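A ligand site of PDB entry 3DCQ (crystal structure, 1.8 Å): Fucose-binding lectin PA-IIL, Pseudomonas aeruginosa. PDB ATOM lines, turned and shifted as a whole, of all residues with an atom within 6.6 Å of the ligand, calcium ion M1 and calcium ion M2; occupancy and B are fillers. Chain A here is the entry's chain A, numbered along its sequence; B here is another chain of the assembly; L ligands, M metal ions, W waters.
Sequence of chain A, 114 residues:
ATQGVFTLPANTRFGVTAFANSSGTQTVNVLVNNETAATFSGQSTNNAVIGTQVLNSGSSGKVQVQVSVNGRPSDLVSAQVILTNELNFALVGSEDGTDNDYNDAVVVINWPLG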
ATOM      1  N   ASN A  21     -19.144 -14.542   9.907  1.00  0.00           N
ATOM      2  CA  ASN A  21     -19.083 -15.989   9.947  1.00  0.00           C
ATOM      3  C   ASN A  21     -20.448 -16.487   9.517  1.00  0.00           C
ATOM      4  O   ASN A  21     -21.222 -16.949  10.327  1.00  0.00           O
ATOM      5  CB  ASN A  21     -18.766 -16.435  11.383  1.00  0.00           C
ATOM      6  CG  ASN A  21     -17.332 -16.132  11.749  1.00  0.00           C
ATOM      7  OD1 ASN A  21     -16.410 -16.834  11.326  1.00  0.00           O
ATOM      8  ND2 ASN A  21     -17.128 -15.059  12.507  1.00  0.00           N
ATOM      9  N   SER A  22     -20.740 -16.378   8.224  1.00  0.00           N
ATOM     10  CA  SER A  22     -22.060 -16.775   7.732  1.00  0.00           C
ATOM     11  C   SER A  22     -22.079 -16.748   6.226  1.00  0.00           C
ATOM     12  O   SER A  22     -21.334 -15.994   5.589  1.00  0.00           O
ATOM     13  CB  SER A  22     -23.127 -15.787   8.238  1.00  0.00           C
ATOM     14  OG  SER A  22     -24.408 -16.087   7.726  1.00  0.00           O
ATOM     15  N   SER A  23     -22.934 -17.588   5.660  1.00  0.00           N
ATOM     16  CA  SER A  23     -23.100 -17.620   4.217  1.00  0.00           C
ATOM     17  C   SER A  23     -23.820 -16.334   3.857  1.00  0.00           C
ATOM     18  O   SER A  23     -23.800 -15.892   2.704  1.00  0.00           O
ATOM     19  CB  SER A  23     -23.975 -18.799   3.798  1.00  0.00           C
ATOM     20  OG  SER A  23     -23.338 -20.022   4.104  1.00  0.00           O
ATOM     21  N   GLY A  24     -24.469 -15.737   4.846  1.00  0.00           N
ATOM     22  CA  GLY A  24     -25.231 -14.523   4.598  1.00  0.00           C
ATOM     23  C   GLY A  24     -24.399 -13.258   4.656  1.00  0.00           C
ATOM     24  O   GLY A  24     -23.485 -13.140   5.471  1.00  0.00           O
ATOM     25  N   THR A  25     -24.708 -12.316   3.772  1.00  0.00           N
ATOM     26  CA  THR A  25     -24.017 -11.047   3.765  1.00  0.00           C
ATOM     27  C   THR A  25     -24.456 -10.290   4.997  1.00  0.00           C
ATOM     28  O   THR A  25     -25.641 -10.103   5.255  1.00  0.00           O
ATOM     29  CB  THR A  25     -24.351 -10.211   2.514  1.00  0.00           C
ATOM     30  OG1 THR A  25     -23.696 -10.796   1.377  1.00  0.00           O
ATOM     31  CG2 THR A  25     -23.875  -8.778   2.693  1.00  0.00           C
ATOM     32  N   GLN A  26     -23.471  -9.855   5.768  1.00  0.00           N
ATOM     33  CA  GLN A  26     -23.725  -9.126   6.980  1.00  0.00           C
ATOM     34  C   GLN A  26     -23.624  -7.630   6.773  1.00  0.00           C
ATOM     35  O   GLN A  26     -22.697  -7.133   6.106  1.00  0.00           O
ATOM     36  CB  GLN A  26     -22.690  -9.501   8.046  1.00  0.00           C
ATOM     37  CG  GLN A  26     -22.566 -10.987   8.299  1.00  0.00           C
ATOM     38  CD  GLN A  26     -23.828 -11.579   8.916  1.00  0.00           C
ATOM     39  OE1 GLN A  26     -24.279 -11.128   9.978  1.00  0.00           O
ATOM     40  NE2 GLN A  26     -24.396 -12.589   8.257  1.00  0.00           N
ATOM     41  N   SER A  44     -18.491 -13.647   4.771  1.00  0.00           N
ATOM     42  CA  SER A  44     -17.400 -14.567   5.039  1.00  0.00           C
ATOM     43  C   SER A  44     -17.848 -15.614   6.021  1.00  0.00           C
ATOM     44  O   SER A  44     -18.632 -15.322   6.912  1.00  0.00           O
ATOM     45  CB  SER A  44     -16.212 -13.842   5.659  1.00  0.00           C
ATOM     46  OG  SER A  44     -15.202 -14.762   6.037  1.00  0.00           O
ATOM     47  N   THR A  45     -17.351 -16.833   5.827  1.00  0.00           N
ATOM     48  CA  THR A  45     -17.608 -17.915   6.779  1.00  0.00           C
ATOM     49  C   THR A  45     -16.244 -18.185   7.416  1.00  0.00           C
ATOM     50  O   THR A  45     -16.038 -19.231   8.011  1.00  0.00           O
ATOM     51  CB  THR A  45     -18.091 -19.188   6.060  1.00  0.00           C
ATOM     52  OG1 THR A  45     -17.276 -19.421   4.909  1.00  0.00           O
ATOM     53  CG2 THR A  45     -19.551 -19.036   5.659  1.00  0.00           C
ATOM     54  N   VAL A  69     -29.228  -8.900   7.909  1.00  0.00           N
ATOM     55  CA  VAL A  69     -28.828  -9.938   6.959  1.00  0.00           C
ATOM     56  C   VAL A  69     -30.073 -10.322   6.161  1.00  0.00           C
ATOM     57  O   VAL A  69     -31.131 -10.590   6.733  1.00  0.00           O
ATOM     58  CB  VAL A  69     -28.333 -11.190   7.683  1.00  0.00           C
ATOM     59  CG1 VAL A  69     -27.863 -12.245   6.659  1.00  0.00           C
ATOM     60  CG2 VAL A  69     -27.208 -10.823   8.660  1.00  0.00           C
ATOM     61  N   ASN A  70     -29.920 -10.363   4.840  1.00  0.00           N
ATOM     62  CA  ASN A  70     -31.030 -10.693   3.986  1.00  0.00           C
ATOM     63  C   ASN A  70     -32.306  -9.992   4.422  1.00  0.00           C
ATOM     64  O   ASN A  70     -33.357 -10.628   4.612  1.00  0.00           O
ATOM     65  CB  ASN A  70     -31.228 -12.220   3.920  1.00  0.00           C
ATOM     66  CG  ASN A  70     -30.171 -12.903   3.052  1.00  0.00           C
ATOM     67  OD1 ASN A  70     -30.299 -14.074   2.666  1.00  0.00           O
ATOM     68  ND2 ASN A  70     -29.125 -12.166   2.737  1.00  0.00           N
ATOM     69  N   SER A  94     -24.281 -11.996  16.889  1.00  0.00           N
ATOM     70  CA  SER A  94     -25.576 -11.883  16.239  1.00  0.00           C
ATOM     71  C   SER A  94     -25.875 -13.164  15.515  1.00  0.00           C
ATOM     72  O   SER A  94     -24.961 -13.830  14.987  1.00  0.00           O
ATOM     73  CB  SER A  94     -25.575 -10.717  15.257  1.00  0.00           C
ATOM     74  OG  SER A  94     -24.529 -10.877  14.329  1.00  0.00           O
ATOM     75  N   GLU A  95     -27.158 -13.497  15.464  1.00  0.00           N
ATOM     76  CA  GLU A  95     -27.619 -14.705  14.809  1.00  0.00           C
ATOM     77  C   GLU A  95     -28.584 -14.326  13.685  1.00  0.00           C
ATOM     78  O   GLU A  95     -29.636 -13.700  13.912  1.00  0.00           O
ATOM     79  CB  GLU A  95     -28.313 -15.596  15.822  1.00  0.00           C
ATOM     80  CG  GLU A  95     -28.917 -16.795  15.180  1.00  0.00           C
ATOM     81  CD  GLU A  95     -27.907 -17.582  14.405  1.00  0.00           C
ATOM     82  OE1 GLU A  95     -26.858 -17.939  14.967  1.00  0.00           O
ATOM     83  OE2 GLU A  95     -28.175 -17.860  13.213  1.00  0.00           O
ATOM     84  N   ASP A  96     -28.208 -14.715  12.474  1.00  0.00           N
ATOM     85  CA  ASP A  96     -29.011 -14.369  11.309  1.00  0.00           C
ATOM     86  C   ASP A  96     -29.943 -15.459  10.863  1.00  0.00           C
ATOM     87  O   ASP A  96     -30.753 -15.238   9.965  1.00  0.00           O
ATOM     88  CB  ASP A  96     -28.118 -13.962  10.132  1.00  0.00           C
ATOM     89  CG  ASP A  96     -27.184 -15.094   9.634  1.00  0.00           C
ATOM     90  OD1 ASP A  96     -27.447 -16.287   9.899  1.00  0.00           O
ATOM     91  OD2 ASP A  96     -26.195 -14.776   8.958  1.00  0.00           O
ATOM     92  N   GLY A  97     -29.827 -16.627  11.477  1.00  0.00           N
ATOM     93  CA  GLY A  97     -30.654 -17.719  11.049  1.00  0.00           C
ATOM     94  C   GLY A  97     -31.196 -18.512  12.194  1.00  0.00           C
ATOM     95  O   GLY A  97     -31.761 -17.959  13.121  1.00  0.00           O
ATOM     96  N   THR A  98     -30.934 -19.821  12.153  1.00  0.00           N
ATOM     97  CA  THR A  98     -31.454 -20.733  13.143  1.00  0.00           C
ATOM     98  C   THR A  98     -30.435 -21.624  13.889  1.00  0.00           C
ATOM     99  O   THR A  98     -30.818 -22.304  14.834  1.00  0.00           O
ATOM    100  CB  THR A  98     -32.461 -21.683  12.475  1.00  0.00           C
ATOM    101  OG1 THR A  98     -31.778 -22.414  11.463  1.00  0.00           O
ATOM    102  CG2 THR A  98     -33.603 -20.897  11.814  1.00  0.00           C
ATOM    103  N   ASP A  99     -29.162 -21.649  13.489  1.00  0.00           N
ATOM    104  CA  ASP A  99     -28.250 -22.548  14.203  1.00  0.00           C
ATOM    105  C   ASP A  99     -27.764 -21.985  15.521  1.00  0.00           C
ATOM    106  O   ASP A  99     -27.160 -22.678  16.326  1.00  0.00           O
ATOM    107  CB  ASP A  99     -27.072 -22.974  13.288  1.00  0.00           C
ATOM    108  CG  ASP A  99     -26.125 -21.847  12.963  1.00  0.00           C
ATOM    109  OD1 ASP A  99     -26.536 -20.696  13.156  1.00  0.00           O
ATOM    110  OD2 ASP A  99     -24.996 -22.108  12.495  1.00  0.00           O
ATOM    111  N   ASN A 100     -28.079 -20.726  15.761  1.00  0.00           N
ATOM    112  CA  ASN A 100     -27.720 -20.069  17.004  1.00  0.00           C
ATOM    113  C   ASN A 100     -26.262 -20.169  17.403  1.00  0.00           C
ATOM    114  O   ASN A 100     -25.964 -20.434  18.571  1.00  0.00           O
ATOM    115  CB  ASN A 100     -28.588 -20.583  18.160  1.00  0.00           C
ATOM    116  CG  ASN A 100     -30.040 -20.185  18.003  1.00  0.00           C
ATOM    117  OD1 ASN A 100     -30.350 -19.214  17.309  1.00  0.00           O
ATOM    118  ND2 ASN A 100     -30.930 -20.901  18.667  1.00  0.00           N
ATOM    119  N   ASP A 101     -25.342 -19.989  16.456  1.00  0.00           N
ATOM    120  CA  ASP A 101     -23.944 -19.970  16.843  1.00  0.00           C
ATOM    121  C   ASP A 101     -23.581 -18.510  17.211  1.00  0.00           C
ATOM    122  O   ASP A 101     -22.535 -18.222  17.804  1.00  0.00           O
ATOM    123  CB  ASP A 101     -23.032 -20.576  15.747  1.00  0.00           C
ATOM    124  CG  ASP A 101     -23.122 -19.871  14.404  1.00  0.00           C
ATOM    125  OD1 ASP A 101     -23.939 -18.949  14.201  1.00  0.00           O
ATOM    126  OD2 ASP A 101     -22.317 -20.243  13.539  1.00  0.00           O
ATOM    127  N   TYR A 102     -24.497 -17.608  16.889  1.00  0.00           N
ATOM    128  CA  TYR A 102     -24.356 -16.187  17.196  1.00  0.00           C
ATOM    129  C   TYR A 102     -23.024 -15.509  16.829  1.00  0.00           C
ATOM    130  O   TYR A 102     -22.639 -14.508  17.448  1.00  0.00           O
ATOM    131  CB  TYR A 102     -24.653 -15.960  18.680  1.00  0.00           C
ATOM    132  CG  TYR A 102     -26.136 -15.926  18.967  1.00  0.00           C
ATOM    133  CD1 TYR A 102     -26.835 -14.712  18.983  1.00  0.00           C
ATOM    134  CD2 TYR A 102     -26.860 -17.121  19.105  1.00  0.00           C
ATOM    135  CE1 TYR A 102     -28.240 -14.675  19.116  1.00  0.00           C
ATOM    136  CE2 TYR A 102     -28.274 -17.086  19.234  1.00  0.00           C
ATOM    137  CZ  TYR A 102     -28.944 -15.863  19.231  1.00  0.00           C
ATOM    138  OH  TYR A 102     -30.330 -15.815  19.286  1.00  0.00           O
ATOM    139  N   ASN A 103     -22.362 -16.016  15.807  1.00  0.00           N
ATOM    140  CA  ASN A 103     -21.093 -15.444  15.363  1.00  0.00           C
ATOM    141  C   ASN A 103     -21.266 -14.903  13.924  1.00  0.00           C
ATOM    142  O   ASN A 103     -20.292 -14.541  13.282  1.00  0.00           O
ATOM    143  CB  ASN A 103     -20.031 -16.529  15.338  1.00  0.00           C
ATOM    144  CG  ASN A 103     -20.286 -17.540  14.223  1.00  0.00           C
ATOM    145  OD1 ASN A 103     -21.312 -17.452  13.566  1.00  0.00           O
ATOM    146  ND2 ASN A 103     -19.370 -18.489  14.014  1.00  0.00           N
ATOM    147  N   ASP A 104     -22.499 -14.836  13.443  1.00  0.00           N
ATOM    148  CA  ASP A 104     -22.718 -14.428  12.060  1.00  0.00           C
ATOM    149  C   ASP A 104     -22.065 -13.096  11.745  1.00  0.00           C
ATOM    150  O   ASP A 104     -21.456 -12.916  10.687  1.00  0.00           O
ATOM    151  CB  ASP A 104     -24.197 -14.487  11.754  1.00  0.00           C
ATOM    152  CG  ASP A 104     -24.729 -15.882  11.985  1.00  0.00           C
ATOM    153  OD1 ASP A 104     -23.954 -16.826  11.711  1.00  0.00           O
ATOM    154  OD2 ASP A 104     -25.877 -16.054  12.452  1.00  0.00           O
ATOM    155  N   ALA A 105     -22.183 -12.172  12.686  1.00  0.00           N
ATOM    156  CA  ALA A 105     -21.506 -10.902  12.608  1.00  0.00           C
ATOM    157  C   ALA A 105     -21.106 -10.760  14.066  1.00  0.00           C
ATOM    158  O   ALA A 105     -21.933 -10.837  14.970  1.00  0.00           O
ATOM    159  CB  ALA A 105     -22.442  -9.769  12.190  1.00  0.00           C
ATOM    160  N   PRO B 112     -16.980 -19.886  18.232  1.00  0.00           N
ATOM    161  CA  PRO B 112     -16.545 -20.605  17.038  1.00  0.00           C
ATOM    162  C   PRO B 112     -16.649 -19.704  15.813  1.00  0.00           C
ATOM    163  O   PRO B 112     -17.247 -18.610  15.879  1.00  0.00           O
ATOM    164  CB  PRO B 112     -17.551 -21.751  16.945  1.00  0.00           C
ATOM    165  CG  PRO B 112     -18.824 -21.059  17.381  1.00  0.00           C
ATOM    166  CD  PRO B 112     -18.342 -20.283  18.628  1.00  0.00           C
ATOM    167  N   LEU B 113     -16.060 -20.154  14.718  1.00  0.00           N
ATOM    168  CA  LEU B 113     -16.139 -19.452  13.455  1.00  0.00           C
ATOM    169  C   LEU B 113     -17.079 -20.239  12.538  1.00  0.00           C
ATOM    170  O   LEU B 113     -17.648 -21.251  12.957  1.00  0.00           O
ATOM    171  CB  LEU B 113     -14.766 -19.367  12.787  1.00  0.00           C
ATOM    172  CG  LEU B 113     -13.635 -18.811  13.638  1.00  0.00           C
ATOM    173  CD1 LEU B 113     -12.373 -18.786  12.774  1.00  0.00           C
ATOM    174  CD2 LEU B 113     -13.986 -17.391  14.122  1.00  0.00           C
ATOM    175  N   GLY B 114     -17.247 -19.745  11.322  1.00  0.00           N
ATOM    176  CA  GLY B 114     -18.057 -20.437  10.332  1.00  0.00           C
ATOM    177  C   GLY B 114     -19.553 -20.199  10.347  1.00  0.00           C
ATOM    178  O   GLY B 114     -20.072 -19.745  11.382  1.00  0.00           O
ATOM    179  OXT GLY B 114     -20.205 -20.487   9.319  1.00  0.00           O
HETATM  180  C1  LIG L   1     -25.687 -19.065   8.026  1.00  0.00           C
HETATM  181  C2  LIG L   1     -25.356 -18.872   9.509  1.00  0.00           C
HETATM  182  O1  LIG L   1     -26.531 -18.527  10.236  1.00  0.00           O
HETATM  183  C3  LIG L   1     -24.772 -20.180  10.063  1.00  0.00           C
HETATM  184  O2  LIG L   1     -24.371 -20.031  11.413  1.00  0.00           O
HETATM  185  C4  LIG L   1     -23.572 -20.596   9.246  1.00  0.00           C
HETATM  186  O3  LIG L   1     -22.533 -19.666   9.443  1.00  0.00           O
HETATM  187  C5  LIG L   1     -23.924 -20.669   7.765  1.00  0.00           C
HETATM  188  O4  LIG L   1     -24.471 -19.400   7.328  1.00  0.00           O
HETATM  189  C6  LIG L   1     -22.693 -20.959   6.929  1.00  0.00           C
HETATM  190  C7  LIG L   1     -26.837 -20.079   7.824  1.00  0.00           C
HETATM  191  C8  LIG L   1     -26.780 -20.291   6.315  1.00  0.00           C
HETATM  192  O5  LIG L   1     -27.029 -19.370   5.537  1.00  0.00           O
HETATM  193  N1  LIG L   1     -26.468 -21.517   5.883  1.00  0.00           N
HETATM  194  C9  LIG L   1     -26.310 -21.812   4.474  1.00  0.00           C
HETATM  195  C10 LIG L   1     -27.318 -21.195   3.507  1.00  0.00           C
HETATM  196  O6  LIG L   1     -26.919 -20.580   2.513  1.00  0.00           O
HETATM  197  C11 LIG L   1     -26.239 -23.321   4.245  1.00  0.00           C
HETATM  198  C12 LIG L   1     -24.869 -23.910   4.552  1.00  0.00           C
HETATM  199  N2  LIG L   1     -28.622 -21.358   3.784  1.00  0.00           N
HETATM  200  C13 LIG L   1     -29.657 -20.806   2.893  1.00  0.00           C
HETATM  201  C14 LIG L   1     -29.676 -19.287   2.741  1.00  0.00           C
HETATM  202  O7  LIG L   1     -30.397 -18.761   1.892  1.00  0.00           O
HETATM  203  C15 LIG L   1     -30.958 -21.346   3.493  1.00  0.00           C
HETATM  204  C16 LIG L   1     -30.616 -21.608   4.941  1.00  0.00           C
HETATM  205  C17 LIG L   1     -29.218 -22.153   4.875  1.00  0.00           C
HETATM  206  N3  LIG L   1     -28.900 -18.594   3.576  1.00  0.00           N
HETATM  207  C18 LIG L   1     -28.803 -17.130   3.525  1.00  0.00           C
HETATM  208  C19 LIG L   1     -27.757 -16.738   2.471  1.00  0.00           C
HETATM  209  O8  LIG L   1     -26.949 -17.625   2.111  1.00  0.00           O
HETATM  210  C20 LIG L   1     -28.375 -16.598   4.891  1.00  0.00           C
HETATM  211  C21 LIG L   1     -29.409 -16.129   5.936  1.00  0.00           C
HETATM  212  C22 LIG L   1     -30.759 -16.741   5.719  1.00  0.00           C
HETATM  213  C23 LIG L   1     -28.864 -16.440   7.312  1.00  0.00           C
HETATM  214  N4  LIG L   1     -27.733 -15.563   2.043  1.00  0.00           N
HETATM  215 CA    CA M   1     -25.813 -18.479  12.737  1.00  0.00          CA
HETATM  216 CA    CA M   2     -22.280 -18.591  11.723  1.00  0.00          CA
HETATM  217  O   HOH W   1     -26.302 -23.507   7.847  1.00  0.00           O
HETATM  218  O   HOH W   2     -28.542 -20.682  10.631  1.00  0.00           O
HETATM  219  O   HOH W   3     -26.734 -12.972   1.769  1.00  0.00           O
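N4 of the ligand lies within hydrogen-bond range of OD1 of Asn 70 (3.0 Å). OD1 of Asp 96 sits close to O1 of the ligand, at 2.4 Å. An oxygen (O4) of the ligand sits close to the side-chain hydroxyl of Ser 23 (3.5 Å). The backbone NH (N) of Ser 23 lies within hydrogen-bond range of an oxygen (O4) of the ligand (2.9 Å). The side-chain hydroxyl of Ser 22 lies close to an oxygen (O4) of the ligand.
The backbone NH (N) of Asn 100 sits close to the side-chain carboxylate (OE1) of Glu 95 (3.1 Å). O of Ser 94 is in hydrogen-bond range of N of Asn 103 (3.5 Å). N of Gly 97 sits close to OE2 of Glu 95. The backbone carbonyl oxygen (O) of Gly 24 sits at hydrogen-bond distance from the side-chain amide nitrogen (NE2) of Gln 26 (3.0 Å). OG of Ser 22 is in hydrogen-bond range of OD2 of Asp 96. The backbone NH (N) of Asp 104 is in hydrogen-bond range of the backbone carbonyl oxygen (O) of Ser 94 (3.1 Å). O of Pro 112 of chain B lies within hydrogen-bond range of ND2 of Asn 103, at 2.8 Å. O of Asp 104 sits close to OE1 of Gln 26, at 3.4 Å.
Residues that only touch the ligand: Gly 24 (3.7 Å) and Thr 45 (3.9 Å). Of the 25 residues printed, 12 come within 4 Å of the ligand. The nearest printed residue that does not touch the ligand is Gly 97 (4.002 Å).
Residues that only touch calcium ion M1: Asp 96. The nearest printed residue that does not touch calcium ion M1 is Asn 100 (4.4 Å).
Five residues have an atom within 4 Å of calcium ion M2: Asn 21, Asp 101, Asn 103, Asp 104 and Gly 114 of chain B. The nearest printed residue that does not touch calcium ion M2 is Ser 22 (4.4 Å).
Calcium ion M1 is bound by OD1 of Asp 99 (2.4 Å), OD1 of Asp 101 (2.4 Å), OD2 of Asp 104 (2.4 Å), OE2 of Glu 95 (2.5 Å), O2 of the ligand (2.5 Å), OE1 of Glu 95 (2.5 Å), O1 of the ligand (2.6 Å) and OD1 of Asp 104 (2.7 Å). Calcium ion M1 has eight donor atoms within binding distance.
Calcium ion M2 is bound by OD1 of Asn 103 (2.4 Å), O of Asn 21 (2.4 Å), OD1 of Asp 104 (2.4 Å), OD2 of Asp 101 (2.5 Å), O of Gly 114 of chain B (2.5 Å), O3 of the ligand (2.5 Å) and O2 of the ligand (2.6 Å). Calcium ion M2 has seven donor atoms within binding distance. Slightly farther from calcium ion M2 lies the side-chain carboxylate (OD1) of Asp 101 (3.0 Å).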
